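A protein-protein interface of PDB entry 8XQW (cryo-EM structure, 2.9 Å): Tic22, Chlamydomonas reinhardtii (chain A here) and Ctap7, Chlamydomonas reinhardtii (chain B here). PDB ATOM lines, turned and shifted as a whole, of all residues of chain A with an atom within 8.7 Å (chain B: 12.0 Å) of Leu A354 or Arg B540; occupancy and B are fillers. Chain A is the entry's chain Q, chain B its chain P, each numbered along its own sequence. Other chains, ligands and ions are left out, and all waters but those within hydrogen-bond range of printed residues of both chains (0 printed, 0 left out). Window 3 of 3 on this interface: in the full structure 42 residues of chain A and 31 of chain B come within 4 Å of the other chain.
Printed residues of chain B within 4 Å of Pro A107: Arg B537.
Printed residues of chain B within 4 Å of Val A226: Ala B544 (3.1 Å) and Tyr B545 (3.7 Å).
Cys A239 touches none of the printed residues of chain B.
Val A350 touches none of the printed residues of chain B.
No residue of chain B comes within 4 Å of Ala A351.
No residue of chain B comes within 4 Å of Pro A352.
Glu A353 touches none of the printed residues of chain B.
Leu A354 touches just one residue of chain B: Arg B540 (3.9 Å).
Of chain B, only Pro B539 (3.9 Å), Arg B540 (3.2 Å) and Tyr B545 (3.9 Å) come within 4 Å of Leu A355.
Arg A356 touches none of the printed residues of chain B.
No residue of chain B comes within 4 Å of Asp A357.
Of the printed residues of chain A, Arg B537 touches Pro A107 (3.6 Å).
Of chain A, only Leu A355 (3.9 Å) comes within 4 Å of Pro B539.
Of chain A, only Leu A354 (3.9 Å) and Leu A355 (3.2 Å) come within 4 Å of Arg B540.
Of the printed residues of chain A, Ala B544 touches Val A226.
Printed residues of chain A within 4 Å of Tyr B545: Val A226 (3.7 Å) and Leu A355 (3.9 Å).
The nearest residue of chain B that does not touch Leu A354 is Pro B539 (4.4 Å).
The nearest residue of chain A that does not touch Arg B540 is Asp A357 (5.2 Å).
The nearest printed residue of chain A that does not touch Arg B537 is Val A226 (5.6 Å).
Pro A107 touches Arg B537.
Ala B544 touches Val A226.
Tyr B545 touches Val A226.
Phe A349 touches Ala B538.
Leu A354 touches Arg B540 (CD1 to CB, 3.9 Å).
CD1 of Leu A355 touches O of Pro B539, 3.9 Å away.
Arg B540 touches Leu A355 (O to CD1, 3.2 Å).
Tyr B545 touches Leu A355 (CE2 to CD1, 3.9 Å).
Of the 19 printed residues of chain A, 5 touch a printed residue of chain B.
Hydrophobic or aromatic side chains of chain A within 4 Å of the printed part of chain B: Pro A107, Val A226, Leu A354 and Leu A355.
Of the 11 printed residues of chain B, 6 touch a printed residue of chain A.
Among the printed residues, no Asp or Glu carboxylate lies within 4 Å of a Lys or Arg side-chain nitrogen of the other chain.
The side-chain carboxylate (OD2) of Asp A242 sits at hydrogen-bond distance from the backbone NH (N) of Leu A355 (2.8 Å).
The side-chain carboxylate (OD2) of Asp A242 sits at hydrogen-bond distance from the backbone NH (N) of Leu A354 (2.8 Å).
O of Pro B539 is in hydrogen-bond range of OH of Tyr B545, 3.3 Å away.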
ATOM      1  N   PRO A 107      21.673 -15.704   3.665  1.00  0.00           N
ATOM      2  CA  PRO A 107      21.396 -17.137   3.461  1.00  0.00           C
ATOM      3  C   PRO A 107      19.927 -17.486   3.276  1.00  0.00           C
ATOM      4  O   PRO A 107      19.621 -18.645   2.971  1.00  0.00           O
ATOM      5  CB  PRO A 107      21.970 -17.782   4.729  1.00  0.00           C
ATOM      6  CG  PRO A 107      23.001 -16.837   5.191  1.00  0.00           C
ATOM      7  CD  PRO A 107      22.438 -15.486   4.904  1.00  0.00           C
ATOM      8  N   VAL A 226      23.912 -22.843  18.238  1.00  0.00           N
ATOM      9  CA  VAL A 226      24.888 -23.562  17.433  1.00  0.00           C
ATOM     10  C   VAL A 226      26.257 -22.944  17.670  1.00  0.00           C
ATOM     11  O   VAL A 226      26.420 -21.719  17.615  1.00  0.00           O
ATOM     12  CB  VAL A 226      24.493 -23.547  15.948  1.00  0.00           C
ATOM     13  CG1 VAL A 226      23.327 -22.601  15.723  1.00  0.00           C
ATOM     14  CG2 VAL A 226      25.682 -23.196  15.059  1.00  0.00           C
ATOM     15  N   LEU A 236      17.886 -18.740  14.231  1.00  0.00           N
ATOM     16  CA  LEU A 236      16.504 -18.325  14.047  1.00  0.00           C
ATOM     17  C   LEU A 236      15.889 -19.152  12.931  1.00  0.00           C
ATOM     18  O   LEU A 236      16.426 -19.198  11.818  1.00  0.00           O
ATOM     19  CB  LEU A 236      16.411 -16.838  13.718  1.00  0.00           C
ATOM     20  CG  LEU A 236      16.027 -15.933  14.882  1.00  0.00           C
ATOM     21  CD1 LEU A 236      17.116 -15.927  15.928  1.00  0.00           C
ATOM     22  CD2 LEU A 236      15.759 -14.537  14.381  1.00  0.00           C
ATOM     23  N   PHE A 237      14.761 -19.792  13.228  1.00  0.00           N
ATOM     24  CA  PHE A 237      14.096 -20.707  12.309  1.00  0.00           C
ATOM     25  C   PHE A 237      12.845 -20.046  11.750  1.00  0.00           C
ATOM     26  O   PHE A 237      11.974 -19.613  12.513  1.00  0.00           O
ATOM     27  CB  PHE A 237      13.724 -22.014  13.005  1.00  0.00           C
ATOM     28  CG  PHE A 237      14.898 -22.784  13.532  1.00  0.00           C
ATOM     29  CD1 PHE A 237      15.552 -22.377  14.675  1.00  0.00           C
ATOM     30  CD2 PHE A 237      15.322 -23.934  12.896  1.00  0.00           C
ATOM     31  CE1 PHE A 237      16.617 -23.091  15.165  1.00  0.00           C
ATOM     32  CE2 PHE A 237      16.388 -24.654  13.383  1.00  0.00           C
ATOM     33  CZ  PHE A 237      17.037 -24.232  14.518  1.00  0.00           C
ATOM     34  N   CYS A 239      10.685 -21.701   9.674  1.00  0.00           N
ATOM     35  CA  CYS A 239       9.667 -22.741   9.682  1.00  0.00           C
ATOM     36  C   CYS A 239       9.788 -23.556  10.960  1.00  0.00           C
ATOM     37  O   CYS A 239      10.878 -24.025  11.305  1.00  0.00           O
ATOM     38  CB  CYS A 239       9.800 -23.660   8.467  1.00  0.00           C
ATOM     39  SG  CYS A 239      11.399 -24.494   8.337  1.00  0.00           S
ATOM     40  N   GLU A 241       8.962 -26.442  11.469  1.00  0.00           N
ATOM     41  CA  GLU A 241       9.269 -27.845  11.209  1.00  0.00           C
ATOM     42  C   GLU A 241      10.740 -28.147  11.472  1.00  0.00           C
ATOM     43  O   GLU A 241      11.074 -29.054  12.244  1.00  0.00           O
ATOM     44  CB  GLU A 241       8.878 -28.194   9.775  1.00  0.00           C
ATOM     45  CG  GLU A 241       7.395 -28.004   9.481  1.00  0.00           C
ATOM     46  CD  GLU A 241       6.504 -28.457  10.625  1.00  0.00           C
ATOM     47  OE1 GLU A 241       5.764 -27.618  11.183  1.00  0.00           O
ATOM     48  OE2 GLU A 241       6.544 -29.658  10.965  1.00  0.00           O
ATOM     49  N   ASP A 242      11.641 -27.399  10.837  1.00  0.00           N
ATOM     50  CA  ASP A 242      13.055 -27.578  11.141  1.00  0.00           C
ATOM     51  C   ASP A 242      13.359 -27.196  12.581  1.00  0.00           C
ATOM     52  O   ASP A 242      14.285 -27.746  13.189  1.00  0.00           O
ATOM     53  CB  ASP A 242      13.912 -26.766  10.174  1.00  0.00           C
ATOM     54  CG  ASP A 242      13.678 -27.157   8.731  1.00  0.00           C
ATOM     55  OD1 ASP A 242      12.547 -27.573   8.411  1.00  0.00           O
ATOM     56  OD2 ASP A 242      14.620 -27.047   7.919  1.00  0.00           O
ATOM     57  N   LEU A 243      12.571 -26.280  13.151  1.00  0.00           N
ATOM     58  CA  LEU A 243      12.728 -25.930  14.556  1.00  0.00           C
ATOM     59  C   LEU A 243      12.630 -27.167  15.441  1.00  0.00           C
ATOM     60  O   LEU A 243      13.566 -27.486  16.185  1.00  0.00           O
ATOM     61  CB  LEU A 243      11.684 -24.888  14.954  1.00  0.00           C
ATOM     62  CG  LEU A 243      11.740 -24.238  16.341  1.00  0.00           C
ATOM     63  CD1 LEU A 243      10.880 -25.007  17.325  1.00  0.00           C
ATOM     64  CD2 LEU A 243      13.166 -24.113  16.854  1.00  0.00           C
ATOM     65  N   ILE A 245      12.617 -30.257  14.432  1.00  0.00           N
ATOM     66  CA  ILE A 245      13.564 -31.257  13.942  1.00  0.00           C
ATOM     67  C   ILE A 245      14.897 -31.117  14.659  1.00  0.00           C
ATOM     68  O   ILE A 245      15.535 -32.113  15.024  1.00  0.00           O
ATOM     69  CB  ILE A 245      13.730 -31.140  12.416  1.00  0.00           C
ATOM     70  CG1 ILE A 245      12.506 -31.705  11.700  1.00  0.00           C
ATOM     71  CG2 ILE A 245      14.983 -31.868  11.962  1.00  0.00           C
ATOM     72  CD1 ILE A 245      12.632 -31.729  10.200  1.00  0.00           C
ATOM     73  N   ALA A 246      15.331 -29.879  14.881  1.00  0.00           N
ATOM     74  CA  ALA A 246      16.557 -29.652  15.632  1.00  0.00           C
ATOM     75  C   ALA A 246      16.355 -29.877  17.126  1.00  0.00           C
ATOM     76  O   ALA A 246      17.186 -30.523  17.776  1.00  0.00           O
ATOM     77  CB  ALA A 246      17.073 -28.237  15.377  1.00  0.00           C
ATOM     78  N   PHE A 349      20.370 -16.827  10.633  1.00  0.00           N
ATOM     79  CA  PHE A 349      19.078 -17.251  10.104  1.00  0.00           C
ATOM     80  C   PHE A 349      19.243 -18.569   9.368  1.00  0.00           C
ATOM     81  O   PHE A 349      20.110 -18.689   8.497  1.00  0.00           O
ATOM     82  CB  PHE A 349      18.503 -16.205   9.153  1.00  0.00           C
ATOM     83  CG  PHE A 349      18.213 -14.890   9.798  1.00  0.00           C
ATOM     84  CD1 PHE A 349      17.009 -14.675  10.439  1.00  0.00           C
ATOM     85  CD2 PHE A 349      19.131 -13.860   9.746  1.00  0.00           C
ATOM     86  CE1 PHE A 349      16.732 -13.463  11.024  1.00  0.00           C
ATOM     87  CE2 PHE A 349      18.859 -12.647  10.329  1.00  0.00           C
ATOM     88  CZ  PHE A 349      17.658 -12.448  10.969  1.00  0.00           C
ATOM     89  N   VAL A 350      18.412 -19.552   9.702  1.00  0.00           N
ATOM     90  CA  VAL A 350      18.461 -20.856   9.055  1.00  0.00           C
ATOM     91  C   VAL A 350      17.515 -20.836   7.865  1.00  0.00           C
ATOM     92  O   VAL A 350      16.539 -20.073   7.845  1.00  0.00           O
ATOM     93  CB  VAL A 350      18.102 -21.987  10.035  1.00  0.00           C
ATOM     94  CG1 VAL A 350      18.746 -21.740  11.387  1.00  0.00           C
ATOM     95  CG2 VAL A 350      16.600 -22.118  10.170  1.00  0.00           C
ATOM     96  N   ALA A 351      17.811 -21.655   6.863  1.00  0.00           N
ATOM     97  CA  ALA A 351      16.998 -21.685   5.665  1.00  0.00           C
ATOM     98  C   ALA A 351      15.751 -22.537   5.889  1.00  0.00           C
ATOM     99  O   ALA A 351      15.826 -23.613   6.484  1.00  0.00           O
ATOM    100  CB  ALA A 351      17.795 -22.239   4.491  1.00  0.00           C
ATOM    101  N   PRO A 352      14.593 -22.071   5.432  1.00  0.00           N
ATOM    102  CA  PRO A 352      13.385 -22.896   5.534  1.00  0.00           C
ATOM    103  C   PRO A 352      13.547 -24.184   4.743  1.00  0.00           C
ATOM    104  O   PRO A 352      14.018 -24.183   3.606  1.00  0.00           O
ATOM    105  CB  PRO A 352      12.292 -22.002   4.944  1.00  0.00           C
ATOM    106  CG  PRO A 352      12.813 -20.613   5.120  1.00  0.00           C
ATOM    107  CD  PRO A 352      14.298 -20.721   4.930  1.00  0.00           C
ATOM    108  N   GLU A 353      13.150 -25.290   5.368  1.00  0.00           N
ATOM    109  CA  GLU A 353      13.295 -26.625   4.794  1.00  0.00           C
ATOM    110  C   GLU A 353      14.747 -26.898   4.406  1.00  0.00           C
ATOM    111  O   GLU A 353      15.059 -27.281   3.278  1.00  0.00           O
ATOM    112  CB  GLU A 353      12.358 -26.820   3.600  1.00  0.00           C
ATOM    113  CG  GLU A 353      11.040 -26.062   3.705  1.00  0.00           C
ATOM    114  CD  GLU A 353      10.237 -26.453   4.928  1.00  0.00           C
ATOM    115  OE1 GLU A 353       9.929 -27.652   5.075  1.00  0.00           O
ATOM    116  OE2 GLU A 353       9.918 -25.566   5.746  1.00  0.00           O
ATOM    117  N   LEU A 354      15.645 -26.686   5.367  1.00  0.00           N
ATOM    118  CA  LEU A 354      17.059 -26.993   5.192  1.00  0.00           C
ATOM    119  C   LEU A 354      17.480 -28.199   6.014  1.00  0.00           C
ATOM    120  O   LEU A 354      18.224 -29.056   5.525  1.00  0.00           O
ATOM    121  CB  LEU A 354      17.913 -25.781   5.572  1.00  0.00           C
ATOM    122  CG  LEU A 354      19.402 -26.004   5.851  1.00  0.00           C
ATOM    123  CD1 LEU A 354      20.129 -26.517   4.622  1.00  0.00           C
ATOM    124  CD2 LEU A 354      20.046 -24.720   6.338  1.00  0.00           C
ATOM    125  N   LEU A 355      17.010 -28.287   7.255  1.00  0.00           N
ATOM    126  CA  LEU A 355      17.405 -29.361   8.150  1.00  0.00           C
ATOM    127  C   LEU A 355      16.774 -30.698   7.794  1.00  0.00           C
ATOM    128  O   LEU A 355      17.237 -31.731   8.285  1.00  0.00           O
ATOM    129  CB  LEU A 355      17.037 -29.010   9.598  1.00  0.00           C
ATOM    130  CG  LEU A 355      17.808 -27.899  10.318  1.00  0.00           C
ATOM    131  CD1 LEU A 355      19.291 -28.193  10.304  1.00  0.00           C
ATOM    132  CD2 LEU A 355      17.529 -26.519   9.736  1.00  0.00           C
ATOM    133  N   ARG A 356      15.734 -30.702   6.959  1.00  0.00           N
ATOM    134  CA  ARG A 356      15.061 -31.946   6.603  1.00  0.00           C
ATOM    135  C   ARG A 356      15.840 -32.704   5.535  1.00  0.00           C
ATOM    136  O   ARG A 356      16.026 -33.922   5.624  1.00  0.00           O
ATOM    137  CB  ARG A 356      13.642 -31.643   6.123  1.00  0.00           C
ATOM    138  CG  ARG A 356      13.116 -30.313   6.623  1.00  0.00           C
ATOM    139  CD  ARG A 356      11.711 -30.043   6.128  1.00  0.00           C
ATOM    140  NE  ARG A 356      10.707 -30.632   7.010  1.00  0.00           N
ATOM    141  CZ  ARG A 356       9.429 -30.270   7.038  1.00  0.00           C
ATOM    142  NH1 ARG A 356       8.984 -29.318   6.230  1.00  0.00           N
ATOM    143  NH2 ARG A 356       8.591 -30.863   7.877  1.00  0.00           N
ATOM    144  N   ASP A 357      16.293 -31.993   4.508  1.00  0.00           N
ATOM    145  CA  ASP A 357      16.973 -32.622   3.386  1.00  0.00           C
ATOM    146  C   ASP A 357      18.475 -32.359   3.424  1.00  0.00           C
ATOM    147  O   ASP A 357      18.979 -31.705   4.337  1.00  0.00           O
ATOM    148  CB  ASP A 357      16.388 -32.121   2.064  1.00  0.00           C
ATOM    149  CG  ASP A 357      14.873 -32.202   2.027  1.00  0.00           C
ATOM    150  OD1 ASP A 357      14.218 -31.274   2.545  1.00  0.00           O
ATOM    151  OD2 ASP A 357      14.338 -33.189   1.480  1.00  0.00           O
ATOM    152  N   GLY B 536      27.329 -15.318  11.156  1.00  0.00           N
ATOM    153  CA  GLY B 536      27.249 -16.758  11.320  1.00  0.00           C
ATOM    154  C   GLY B 536      26.469 -17.422  10.198  1.00  0.00           C
ATOM    155  O   GLY B 536      25.406 -16.958   9.788  1.00  0.00           O
ATOM    156  N   ARG B 537      27.009 -18.535   9.710  1.00  0.00           N
ATOM    157  CA  ARG B 537      26.412 -19.312   8.631  1.00  0.00           C
ATOM    158  C   ARG B 537      25.836 -20.592   9.221  1.00  0.00           C
ATOM    159  O   ARG B 537      26.567 -21.389   9.819  1.00  0.00           O
ATOM    160  CB  ARG B 537      27.444 -19.622   7.551  1.00  0.00           C
ATOM    161  CG  ARG B 537      26.833 -20.060   6.240  1.00  0.00           C
ATOM    162  CD  ARG B 537      26.169 -18.895   5.529  1.00  0.00           C
ATOM    163  NE  ARG B 537      27.137 -17.870   5.157  1.00  0.00           N
ATOM    164  CZ  ARG B 537      27.183 -16.656   5.692  1.00  0.00           C
ATOM    165  NH1 ARG B 537      26.308 -16.308   6.624  1.00  0.00           N
ATOM    166  NH2 ARG B 537      28.100 -15.787   5.290  1.00  0.00           N
ATOM    167  N   ALA B 538      24.534 -20.790   9.052  1.00  0.00           N
ATOM    168  CA  ALA B 538      23.872 -21.921   9.682  1.00  0.00           C
ATOM    169  C   ALA B 538      24.294 -23.228   9.015  1.00  0.00           C
ATOM    170  O   ALA B 538      24.447 -23.278   7.790  1.00  0.00           O
ATOM    171  CB  ALA B 538      22.355 -21.761   9.610  1.00  0.00           C
ATOM    172  N   PRO B 539      24.497 -24.294   9.783  1.00  0.00           N
ATOM    173  CA  PRO B 539      24.859 -25.590   9.199  1.00  0.00           C
ATOM    174  C   PRO B 539      23.646 -26.479   8.968  1.00  0.00           C
ATOM    175  O   PRO B 539      22.583 -26.294   9.560  1.00  0.00           O
ATOM    176  CB  PRO B 539      25.783 -26.193  10.265  1.00  0.00           C
ATOM    177  CG  PRO B 539      25.358 -25.533  11.564  1.00  0.00           C
ATOM    178  CD  PRO B 539      24.486 -24.342  11.252  1.00  0.00           C
ATOM    179  N   ARG B 540      23.818 -27.465   8.083  1.00  0.00           N
ATOM    180  CA  ARG B 540      22.717 -28.376   7.784  1.00  0.00           C
ATOM    181  C   ARG B 540      22.719 -29.590   8.702  1.00  0.00           C
ATOM    182  O   ARG B 540      21.657 -30.020   9.161  1.00  0.00           O
ATOM    183  CB  ARG B 540      22.770 -28.815   6.320  1.00  0.00           C
ATOM    184  CG  ARG B 540      24.060 -29.480   5.900  1.00  0.00           C
ATOM    185  CD  ARG B 540      24.370 -29.154   4.461  1.00  0.00           C
ATOM    186  NE  ARG B 540      24.645 -27.734   4.297  1.00  0.00           N
ATOM    187  CZ  ARG B 540      24.184 -26.998   3.296  1.00  0.00           C
ATOM    188  NH1 ARG B 540      23.417 -27.552   2.371  1.00  0.00           N
ATOM    189  NH2 ARG B 540      24.482 -25.710   3.222  1.00  0.00           N
ATOM    190  N   ASP B 541      23.885 -30.172   8.966  1.00  0.00           N
ATOM    191  CA  ASP B 541      23.952 -31.311   9.871  1.00  0.00           C
ATOM    192  C   ASP B 541      23.691 -30.853  11.297  1.00  0.00           C
ATOM    193  O   ASP B 541      24.291 -29.883  11.766  1.00  0.00           O
ATOM    194  CB  ASP B 541      25.312 -31.996   9.782  1.00  0.00           C
ATOM    195  CG  ASP B 541      25.421 -33.188  10.711  1.00  0.00           C
ATOM    196  OD1 ASP B 541      24.377 -33.809  11.001  1.00  0.00           O
ATOM    197  OD2 ASP B 541      26.543 -33.507  11.154  1.00  0.00           O
ATOM    198  N   VAL B 542      22.810 -31.562  11.995  1.00  0.00           N
ATOM    199  CA  VAL B 542      22.447 -31.186  13.367  1.00  0.00           C
ATOM    200  C   VAL B 542      23.510 -31.813  14.261  1.00  0.00           C
ATOM    201  O   VAL B 542      23.365 -32.905  14.817  1.00  0.00           O
ATOM    202  CB  VAL B 542      21.016 -31.607  13.726  1.00  0.00           C
ATOM    203  CG1 VAL B 542      20.741 -33.050  13.301  1.00  0.00           C
ATOM    204  CG2 VAL B 542      20.735 -31.388  15.215  1.00  0.00           C
ATOM    205  N   ALA B 543      24.632 -31.110  14.373  1.00  0.00           N
ATOM    206  CA  ALA B 543      25.697 -31.495  15.283  1.00  0.00           C
ATOM    207  C   ALA B 543      26.191 -30.343  16.137  1.00  0.00           C
ATOM    208  O   ALA B 543      26.590 -30.581  17.280  1.00  0.00           O
ATOM    209  CB  ALA B 543      26.880 -32.091  14.505  1.00  0.00           C
ATOM    210  N   ALA B 544      26.170 -29.109  15.640  1.00  0.00           N
ATOM    211  CA  ALA B 544      26.523 -27.951  16.440  1.00  0.00           C
ATOM    212  C   ALA B 544      25.343 -27.410  17.227  1.00  0.00           C
ATOM    213  O   ALA B 544      25.533 -26.536  18.078  1.00  0.00           O
ATOM    214  CB  ALA B 544      27.092 -26.839  15.555  1.00  0.00           C
ATOM    215  N   TYR B 545      24.137 -27.911  16.972  1.00  0.00           N
ATOM    216  CA  TYR B 545      22.970 -27.527  17.754  1.00  0.00           C
ATOM    217  C   TYR B 545      23.111 -28.203  19.112  1.00  0.00           C
ATOM    218  O   TYR B 545      22.677 -29.335  19.336  1.00  0.00           O
ATOM    219  CB  TYR B 545      21.689 -27.919  17.036  1.00  0.00           C
ATOM    220  CG  TYR B 545      21.490 -27.184  15.730  1.00  0.00           C
ATOM    221  CD1 TYR B 545      21.129 -25.845  15.718  1.00  0.00           C
ATOM    222  CD2 TYR B 545      21.659 -27.827  14.513  1.00  0.00           C
ATOM    223  CE1 TYR B 545      20.947 -25.168  14.533  1.00  0.00           C
ATOM    224  CE2 TYR B 545      21.476 -27.156  13.321  1.00  0.00           C
ATOM    225  CZ  TYR B 545      21.119 -25.827  13.339  1.00  0.00           C
ATOM    226  OH  TYR B 545      20.936 -25.151  12.155  1.00  0.00           O
ATOM    227  N   THR B 546      23.755 -27.485  20.032  1.00  0.00           N
ATOM    228  CA  THR B 546      24.226 -28.110  21.265  1.00  0.00           C
ATOM    229  C   THR B 546      23.102 -28.283  22.279  1.00  0.00           C
ATOM    230  O   THR B 546      22.883 -29.385  22.793  1.00  0.00           O
ATOM    231  CB  THR B 546      25.367 -27.287  21.860  1.00  0.00           C
ATOM    232  OG1 THR B 546      25.068 -25.894  21.724  1.00  0.00           O
ATOM    233  CG2 THR B 546      26.676 -27.602  21.151  1.00  0.00           C
